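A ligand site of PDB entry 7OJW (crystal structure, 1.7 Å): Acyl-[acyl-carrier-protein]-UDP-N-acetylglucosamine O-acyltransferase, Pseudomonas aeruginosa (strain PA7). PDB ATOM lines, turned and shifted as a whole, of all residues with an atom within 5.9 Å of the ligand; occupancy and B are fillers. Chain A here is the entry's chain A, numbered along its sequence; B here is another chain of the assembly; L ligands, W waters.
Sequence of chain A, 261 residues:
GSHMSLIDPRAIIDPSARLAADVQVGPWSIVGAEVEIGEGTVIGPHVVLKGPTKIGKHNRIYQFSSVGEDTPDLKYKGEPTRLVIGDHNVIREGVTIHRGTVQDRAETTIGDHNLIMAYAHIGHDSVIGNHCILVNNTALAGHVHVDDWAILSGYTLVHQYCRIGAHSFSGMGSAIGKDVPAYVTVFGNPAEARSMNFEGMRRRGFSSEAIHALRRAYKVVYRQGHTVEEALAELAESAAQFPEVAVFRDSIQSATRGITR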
ATOM      1  N   LEU A 115     -14.232 -10.209  25.611  1.00  0.00           N
ATOM      2  CA  LEU A 115     -14.428  -9.189  24.589  1.00  0.00           C
ATOM      3  C   LEU A 115     -14.836  -9.947  23.350  1.00  0.00           C
ATOM      4  O   LEU A 115     -14.057 -10.759  22.848  1.00  0.00           O
ATOM      5  CB  LEU A 115     -13.140  -8.394  24.358  1.00  0.00           C
ATOM      6  CG  LEU A 115     -13.149  -7.440  23.140  1.00  0.00           C
ATOM      7  CD1 LEU A 115     -14.388  -6.471  23.170  1.00  0.00           C
ATOM      8  CD2 LEU A 115     -11.838  -6.660  23.075  1.00  0.00           C
ATOM      9  N   MET A 117     -16.060  -9.335  19.677  1.00  0.00           N
ATOM     10  CA  MET A 117     -15.988  -8.243  18.728  1.00  0.00           C
ATOM     11  C   MET A 117     -16.986  -8.379  17.625  1.00  0.00           C
ATOM     12  O   MET A 117     -17.705  -9.378  17.556  1.00  0.00           O
ATOM     13  CB  MET A 117     -14.540  -8.054  18.235  1.00  0.00           C
ATOM     14  CG  MET A 117     -13.638  -7.651  19.420  1.00  0.00           C
ATOM     15  SD  MET A 117     -11.889  -7.518  19.030  1.00  0.00           S
ATOM     16  CE  MET A 117     -11.868  -6.080  18.101  1.00  0.00           C
ATOM     17  N   ILE A 133     -10.753 -13.224  24.028  1.00  0.00           N
ATOM     18  CA  ILE A 133     -10.984 -12.225  22.990  1.00  0.00           C
ATOM     19  C   ILE A 133     -11.375 -12.967  21.743  1.00  0.00           C
ATOM     20  O   ILE A 133     -10.555 -13.751  21.247  1.00  0.00           O
ATOM     21  CB  ILE A 133      -9.802 -11.273  22.739  1.00  0.00           C
ATOM     22  CG1 ILE A 133      -9.334 -10.586  24.045  1.00  0.00           C
ATOM     23  CG2 ILE A 133     -10.193 -10.222  21.645  1.00  0.00           C
ATOM     24  CD1 ILE A 133      -8.100  -9.670  23.947  1.00  0.00           C
ATOM     25  N   VAL A 135     -12.174 -12.042  18.115  1.00  0.00           N
ATOM     26  CA  VAL A 135     -12.067 -10.859  17.240  1.00  0.00           C
ATOM     27  C   VAL A 135     -13.171 -10.932  16.190  1.00  0.00           C
ATOM     28  O   VAL A 135     -13.780 -11.984  16.020  1.00  0.00           O
ATOM     29  CB  VAL A 135     -10.599 -10.711  16.665  1.00  0.00           C
ATOM     30  CG1 VAL A 135     -10.442  -9.438  15.844  1.00  0.00           C
ATOM     31  CG2 VAL A 135      -9.581 -10.696  17.823  1.00  0.00           C
ATOM     32  N   ASN A 136     -13.403  -9.821  15.486  1.00  0.00           N
ATOM     33  CA  ASN A 136     -14.451  -9.685  14.449  1.00  0.00           C
ATOM     34  C   ASN A 136     -14.665 -10.919  13.635  1.00  0.00           C
ATOM     35  O   ASN A 136     -13.694 -11.473  13.092  1.00  0.00           O
ATOM     36  CB  ASN A 136     -14.058  -8.606  13.443  1.00  0.00           C
ATOM     37  CG  ASN A 136     -14.006  -7.225  13.995  1.00  0.00           C
ATOM     38  OD1 ASN A 136     -13.409  -6.993  15.027  1.00  0.00           O
ATOM     39  ND2 ASN A 136     -14.576  -6.277  13.267  1.00  0.00           N
ATOM     40  N   ILE A 151      -7.197 -16.183  22.541  1.00  0.00           N
ATOM     41  CA  ILE A 151      -7.434 -15.061  21.591  1.00  0.00           C
ATOM     42  C   ILE A 151      -7.651 -15.690  20.232  1.00  0.00           C
ATOM     43  O   ILE A 151      -6.769 -16.407  19.753  1.00  0.00           O
ATOM     44  CB  ILE A 151      -6.244 -14.066  21.548  1.00  0.00           C
ATOM     45  CG1 ILE A 151      -6.088 -13.311  22.887  1.00  0.00           C
ATOM     46  CG2 ILE A 151      -6.387 -13.063  20.357  1.00  0.00           C
ATOM     47  CD1 ILE A 151      -4.707 -12.603  23.020  1.00  0.00           C
ATOM     48  N   LEU A 152      -8.817 -15.456  19.620  1.00  0.00           N
ATOM     49  CA  LEU A 152      -9.092 -15.977  18.278  1.00  0.00           C
ATOM     50  C   LEU A 152      -9.102 -14.770  17.375  1.00  0.00           C
ATOM     51  O   LEU A 152      -9.989 -13.919  17.546  1.00  0.00           O
ATOM     52  CB  LEU A 152     -10.426 -16.740  18.242  1.00  0.00           C
ATOM     53  CG  LEU A 152     -10.496 -17.968  19.187  1.00  0.00           C
ATOM     54  CD1 LEU A 152     -11.855 -18.651  19.133  1.00  0.00           C
ATOM     55  CD2 LEU A 152      -9.435 -19.030  18.829  1.00  0.00           C
ATOM     56  N   SER A 153      -8.128 -14.650  16.461  1.00  0.00           N
ATOM     57  CA  SER A 153      -8.019 -13.452  15.598  1.00  0.00           C
ATOM     58  C   SER A 153      -9.197 -13.384  14.625  1.00  0.00           C
ATOM     59  O   SER A 153      -9.951 -14.363  14.519  1.00  0.00           O
ATOM     60  CB  SER A 153      -6.687 -13.410  14.855  1.00  0.00           C
ATOM     61  OG  SER A 153      -5.602 -13.279  15.799  1.00  0.00           O
ATOM     62  N   GLY A 154      -9.349 -12.233  13.922  1.00  0.00           N
ATOM     63  CA  GLY A 154     -10.495 -11.957  13.052  1.00  0.00           C
ATOM     64  C   GLY A 154     -10.730 -13.067  12.078  1.00  0.00           C
ATOM     65  O   GLY A 154      -9.770 -13.630  11.531  1.00  0.00           O
ATOM     66  N   TYR A 155     -12.014 -13.415  11.902  1.00  0.00           N
ATOM     67  CA  TYR A 155     -12.471 -14.430  10.959  1.00  0.00           C
ATOM     68  C   TYR A 155     -11.949 -15.836  11.251  1.00  0.00           C
ATOM     69  O   TYR A 155     -11.869 -16.654  10.335  1.00  0.00           O
ATOM     70  CB  TYR A 155     -12.164 -13.965   9.513  1.00  0.00           C
ATOM     71  CG  TYR A 155     -13.043 -12.807   9.080  1.00  0.00           C
ATOM     72  CD1 TYR A 155     -12.821 -11.517   9.571  1.00  0.00           C
ATOM     73  CD2 TYR A 155     -14.083 -12.999   8.191  1.00  0.00           C
ATOM     74  CE1 TYR A 155     -13.611 -10.446   9.154  1.00  0.00           C
ATOM     75  CE2 TYR A 155     -14.897 -11.943   7.798  1.00  0.00           C
ATOM     76  CZ  TYR A 155     -14.670 -10.673   8.297  1.00  0.00           C
ATOM     77  OH  TYR A 155     -15.513  -9.676   7.854  1.00  0.00           O
ATOM     78  N   PHE A 169      -3.781 -19.111  20.823  1.00  0.00           N
ATOM     79  CA  PHE A 169      -3.990 -17.973  19.931  1.00  0.00           C
ATOM     80  C   PHE A 169      -4.191 -18.505  18.523  1.00  0.00           C
ATOM     81  O   PHE A 169      -3.438 -19.405  18.108  1.00  0.00           O
ATOM     82  CB  PHE A 169      -2.688 -17.084  19.973  1.00  0.00           C
ATOM     83  CG  PHE A 169      -2.630 -16.005  18.911  1.00  0.00           C
ATOM     84  CD1 PHE A 169      -3.158 -14.740  19.154  1.00  0.00           C
ATOM     85  CD2 PHE A 169      -2.096 -16.266  17.646  1.00  0.00           C
ATOM     86  CE1 PHE A 169      -3.123 -13.745  18.156  1.00  0.00           C
ATOM     87  CE2 PHE A 169      -2.057 -15.269  16.661  1.00  0.00           C
ATOM     88  CZ  PHE A 169      -2.590 -14.025  16.916  1.00  0.00           C
ATOM     89  N   MET A 172      -5.347 -14.679  11.945  1.00  0.00           N
ATOM     90  CA  MET A 172      -6.577 -14.274  11.254  1.00  0.00           C
ATOM     91  C   MET A 172      -6.929 -15.289  10.175  1.00  0.00           C
ATOM     92  O   MET A 172      -6.026 -15.906   9.594  1.00  0.00           O
ATOM     93  CB  MET A 172      -6.424 -12.842  10.673  1.00  0.00           C
ATOM     94  CG  MET A 172      -5.492 -12.778   9.541  1.00  0.00           C
ATOM     95  SD  MET A 172      -5.329 -11.080   8.943  1.00  0.00           S
ATOM     96  CE  MET A 172      -4.398 -11.401   7.551  1.00  0.00           C
ATOM     97  N   PRO B  72      -9.753   1.106  19.606  1.00  0.00           N
ATOM     98  CA  PRO B  72      -9.335   0.202  20.701  1.00  0.00           C
ATOM     99  C   PRO B  72      -7.941   0.489  21.269  1.00  0.00           C
ATOM    100  O   PRO B  72      -6.978   0.639  20.533  1.00  0.00           O
ATOM    101  CB  PRO B  72      -9.438  -1.207  20.079  1.00  0.00           C
ATOM    102  CG  PRO B  72      -9.335  -0.987  18.609  1.00  0.00           C
ATOM    103  CD  PRO B  72      -9.828   0.401  18.304  1.00  0.00           C
ATOM    104  N   HIS B 121     -14.997  -3.867   7.321  1.00  0.00           N
ATOM    105  CA  HIS B 121     -14.530  -3.299   8.584  1.00  0.00           C
ATOM    106  C   HIS B 121     -13.273  -2.459   8.334  1.00  0.00           C
ATOM    107  O   HIS B 121     -12.295  -2.946   7.734  1.00  0.00           O
ATOM    108  CB  HIS B 121     -14.175  -4.408   9.578  1.00  0.00           C
ATOM    109  CG  HIS B 121     -13.489  -3.900  10.813  1.00  0.00           C
ATOM    110  ND1 HIS B 121     -14.198  -3.232  11.790  1.00  0.00           N
ATOM    111  CD2 HIS B 121     -12.193  -3.963  11.161  1.00  0.00           C
ATOM    112  CE1 HIS B 121     -13.313  -2.946  12.750  1.00  0.00           C
ATOM    113  NE2 HIS B 121     -12.080  -3.325  12.394  1.00  0.00           N
ATOM    114  N   HIS B 124      -9.141   1.205  13.238  1.00  0.00           N
ATOM    115  CA  HIS B 124      -8.533   2.440  13.665  1.00  0.00           C
ATOM    116  C   HIS B 124      -7.254   2.812  12.930  1.00  0.00           C
ATOM    117  O   HIS B 124      -6.390   1.957  12.684  1.00  0.00           O
ATOM    118  CB  HIS B 124      -8.249   2.406  15.186  1.00  0.00           C
ATOM    119  CG  HIS B 124      -7.241   1.379  15.607  1.00  0.00           C
ATOM    120  ND1 HIS B 124      -7.579   0.041  15.731  1.00  0.00           N
ATOM    121  CD2 HIS B 124      -5.929   1.527  15.905  1.00  0.00           C
ATOM    122  CE1 HIS B 124      -6.469  -0.576  16.108  1.00  0.00           C
ATOM    123  NE2 HIS B 124      -5.450   0.270  16.242  1.00  0.00           N
ATOM    124  N   ALA B 139     -11.807  -6.831   5.774  1.00  0.00           N
ATOM    125  CA  ALA B 139     -11.544  -6.305   7.111  1.00  0.00           C
ATOM    126  C   ALA B 139     -10.112  -5.812   7.170  1.00  0.00           C
ATOM    127  O   ALA B 139      -9.167  -6.537   6.822  1.00  0.00           O
ATOM    128  CB  ALA B 139     -11.776  -7.387   8.159  1.00  0.00           C
ATOM    129  N   LEU B 140      -9.965  -4.532   7.520  1.00  0.00           N
ATOM    130  CA  LEU B 140      -8.650  -3.902   7.684  1.00  0.00           C
ATOM    131  C   LEU B 140      -8.440  -3.868   9.196  1.00  0.00           C
ATOM    132  O   LEU B 140      -9.177  -3.181   9.889  1.00  0.00           O
ATOM    133  CB  LEU B 140      -8.647  -2.458   7.132  1.00  0.00           C
ATOM    134  CG  LEU B 140      -9.174  -2.284   5.687  1.00  0.00           C
ATOM    135  CD1 LEU B 140      -8.959  -0.837   5.242  1.00  0.00           C
ATOM    136  CD2 LEU B 140      -8.481  -3.246   4.733  1.00  0.00           C
ATOM    137  N   ALA B 141      -7.447  -4.610   9.693  1.00  0.00           N
ATOM    138  CA  ALA B 141      -7.240  -4.710  11.150  1.00  0.00           C
ATOM    139  C   ALA B 141      -6.988  -3.401  11.875  1.00  0.00           C
ATOM    140  O   ALA B 141      -7.450  -3.214  13.009  1.00  0.00           O
ATOM    141  CB  ALA B 141      -6.118  -5.696  11.477  1.00  0.00           C
ATOM    142  N   GLY B 142      -6.246  -2.495  11.249  1.00  0.00           N
ATOM    143  CA  GLY B 142      -5.852  -1.252  11.903  1.00  0.00           C
ATOM    144  C   GLY B 142      -4.548  -0.761  11.322  1.00  0.00           C
ATOM    145  O   GLY B 142      -3.708  -1.585  10.908  1.00  0.00           O
ATOM    146  N   LEU B 157      -8.793 -10.218   4.167  1.00  0.00           N
ATOM    147  CA  LEU B 157      -8.329  -9.858   5.519  1.00  0.00           C
ATOM    148  C   LEU B 157      -6.963  -9.189   5.424  1.00  0.00           C
ATOM    149  O   LEU B 157      -6.052  -9.692   4.742  1.00  0.00           O
ATOM    150  CB  LEU B 157      -8.196 -11.133   6.357  1.00  0.00           C
ATOM    151  CG  LEU B 157      -9.416 -12.046   6.398  1.00  0.00           C
ATOM    152  CD1 LEU B 157      -9.140 -13.319   7.222  1.00  0.00           C
ATOM    153  CD2 LEU B 157     -10.640 -11.252   6.887  1.00  0.00           C
ATOM    154  N   VAL B 158      -6.820  -8.043   6.085  1.00  0.00           N
ATOM    155  CA  VAL B 158      -5.553  -7.326   6.028  1.00  0.00           C
ATOM    156  C   VAL B 158      -4.990  -7.125   7.440  1.00  0.00           C
ATOM    157  O   VAL B 158      -5.630  -6.497   8.290  1.00  0.00           O
ATOM    158  CB  VAL B 158      -5.663  -6.006   5.244  1.00  0.00           C
ATOM    159  CG1 VAL B 158      -4.288  -5.387   5.063  1.00  0.00           C
ATOM    160  CG2 VAL B 158      -6.351  -6.206   3.870  1.00  0.00           C
ATOM    161  N   HIS B 159      -3.785  -7.630   7.653  1.00  0.00           N
ATOM    162  CA  HIS B 159      -3.051  -7.515   8.914  1.00  0.00           C
ATOM    163  C   HIS B 159      -2.746  -6.060   9.222  1.00  0.00           C
ATOM    164  O   HIS B 159      -2.601  -5.248   8.313  1.00  0.00           O
ATOM    165  CB  HIS B 159      -1.720  -8.296   8.770  1.00  0.00           C
ATOM    166  CG  HIS B 159      -0.942  -8.452  10.047  1.00  0.00           C
ATOM    167  ND1 HIS B 159      -0.124  -7.441  10.532  1.00  0.00           N
ATOM    168  CD2 HIS B 159      -0.791  -9.552  10.833  1.00  0.00           C
ATOM    169  CE1 HIS B 159       0.434  -7.909  11.643  1.00  0.00           C
ATOM    170  NE2 HIS B 159       0.096  -9.188  11.856  1.00  0.00           N
ATOM    171  N   GLN B 160      -2.664  -5.712  10.528  1.00  0.00           N
ATOM    172  CA  GLN B 160      -2.317  -4.363  10.935  1.00  0.00           C
ATOM    173  C   GLN B 160      -1.016  -3.895  10.269  1.00  0.00           C
ATOM    174  O   GLN B 160      -0.118  -4.697  10.080  1.00  0.00           O
ATOM    175  CB  GLN B 160      -2.030  -4.332  12.454  1.00  0.00           C
ATOM    176  CG  GLN B 160      -3.283  -4.269  13.278  1.00  0.00           C
ATOM    177  CD  GLN B 160      -2.931  -3.804  14.679  1.00  0.00           C
ATOM    178  OE1 GLN B 160      -2.215  -4.480  15.421  1.00  0.00           O
ATOM    179  NE2 GLN B 160      -3.434  -2.639  15.033  1.00  0.00           N
HETATM  180  C1  LIG L   1     -10.593  -6.815  12.990  1.00  0.00           C
HETATM  181  C2  LIG L   1      -9.596  -6.686  13.953  1.00  0.00           C
HETATM  182  C3  LIG L   1     -10.452  -7.676  11.920  1.00  0.00           C
HETATM  183  C4  LIG L   1      -5.897  -9.093  19.603  1.00  0.00           C
HETATM  184  C5  LIG L   1      -7.276  -8.088  17.935  1.00  0.00           C
HETATM  185  C6  LIG L   1      -6.461  -8.231  20.533  1.00  0.00           C
HETATM  186  C7  LIG L   1      -7.812  -7.224  18.855  1.00  0.00           C
HETATM  187  C8  LIG L   1      -8.446  -7.453  13.840  1.00  0.00           C
HETATM  188  C9  LIG L   1      -9.238  -4.910  21.869  1.00  0.00           C
HETATM  189  C10 LIG L   1      -7.812  -6.361  22.438  1.00  0.00           C
HETATM  190  C11 LIG L   1      -6.333  -9.024  18.280  1.00  0.00           C
HETATM  191  C12 LIG L   1      -9.301  -8.435  11.813  1.00  0.00           C
HETATM  192  C13 LIG L   1      -7.419  -7.306  20.171  1.00  0.00           C
HETATM  193  C14 LIG L   1      -8.301  -8.342  12.773  1.00  0.00           C
HETATM  194  C15 LIG L   1      -4.870  -6.996  16.133  1.00  0.00           C
HETATM  195  C16 LIG L   1      -6.415  -9.587  14.866  1.00  0.00           C
HETATM  196  C17 LIG L   1      -8.271  -8.740   9.571  1.00  0.00           C
HETATM  197  C18 LIG L   1      -4.533  -5.285  17.827  1.00  0.00           C
HETATM  198  C19 LIG L   1      -9.127  -9.372  10.655  1.00  0.00           C
HETATM  199  C20 LIG L   1      -5.769  -9.934  17.231  1.00  0.00           C
HETATM  200  C21 LIG L   1      -4.431  -8.374  15.738  1.00  0.00           C
HETATM  201  C22 LIG L   1      -6.103  -8.932  13.533  1.00  0.00           C
HETATM  202  N1  LIG L   1      -8.569  -5.423  22.953  1.00  0.00           N
HETATM  203  N2  LIG L   1      -8.930  -5.513  20.712  1.00  0.00           N
HETATM  204  N3  LIG L   1      -8.018  -6.435  21.095  1.00  0.00           N
HETATM  205  N4  LIG L   1      -4.225  -6.589  17.275  1.00  0.00           N
HETATM  206  N5  LIG L   1      -5.574  -9.254  15.937  1.00  0.00           N
HETATM  207  O1  LIG L   1      -5.729  -6.354  15.528  1.00  0.00           O
HETATM  208  O2  LIG L   1      -7.328 -10.387  14.985  1.00  0.00           O
HETATM  209  O3  LIG L   1      -7.202  -9.178  12.610  1.00  0.00           O
HETATM  210  O   HOH W   1      -3.028  -7.744  12.515  1.00  0.00           O
HETATM  211  O   HOH W   2      -7.078  -4.028  15.588  1.00  0.00           O
HETATM  212  O   HOH W   3      -2.376  -7.728  19.119  1.00  0.00           O
HETATM  213  O   HOH W   4      -3.762 -11.586  14.605  1.00  0.00           O
HETATM  214  O   HOH W   5      -3.796 -10.171  11.557  1.00  0.00           O
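The backbone NH (N) of Ala 141 of chain B is in hydrogen-bond range of the backbone carbonyl oxygen (O) of Val 158 of chain B. The side-chain amide nitrogen of Asn 136 lies within hydrogen-bond range of a ring nitrogen (ND1) of His 121 of chain B (3.4 Å). The backbone carbonyl oxygen of Ile 133 lies within hydrogen-bond range of the backbone NH of Leu 152, 2.9 Å away. O of Asn 136 lies within hydrogen-bond range of N of Tyr 155 (2.8 Å). The backbone carbonyl oxygen (O) of His 121 of chain B sits at hydrogen-bond distance from the backbone NH (N) of Leu 140 of chain B, at 2.8 Å. The backbone NH (N) of Val 135 lies within hydrogen-bond range of the backbone carbonyl oxygen (O) of Leu 152 (2.9 Å). The backbone carbonyl oxygen (O) of Ala 139 of chain B is in hydrogen-bond range of the backbone NH (N) of Val 158 of chain B (2.9 Å).
The side-chain hydroxyl of Ser 153 sits close to an oxygen (O2) of the ligand (3.5 Å). The side-chain amide oxygen (OE1) of Gln 160 of chain B sits close to a nitrogen (N4) of the ligand (3.5 Å). O2 of the ligand lies within hydrogen-bond range of N of Gly 154 (2.9 Å).
Water W2 lies within hydrogen-bond range of O1 of the ligand (2.7 Å) and O of Ala 141 of chain B (2.7 Å).
Merely in contact with the ligand: Leu 115, Val 135, Asn 136, Ala 139 of chain B, Ile 133, Ala 141 of chain B, Val 158 of chain B, His 121 of chain B, Met 172 and Met 117. Hydrophobic or aromatic side chains that line the ligand: Leu 115, Met 117, Ile 133, Val 135, Met 172, His 121 of chain B, Ala 139 of chain B and Ala 141 of chain B. Within 4 Å of the ligand: Leu 115, Met 117, Ile 133, Val 135, Asn 136, Ser 153, Gly 154, Met 172, His 121 of chain B, Ala 139 of chain B, Ala 141 of chain B, Val 158 of chain B and Gln 160 of chain B.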
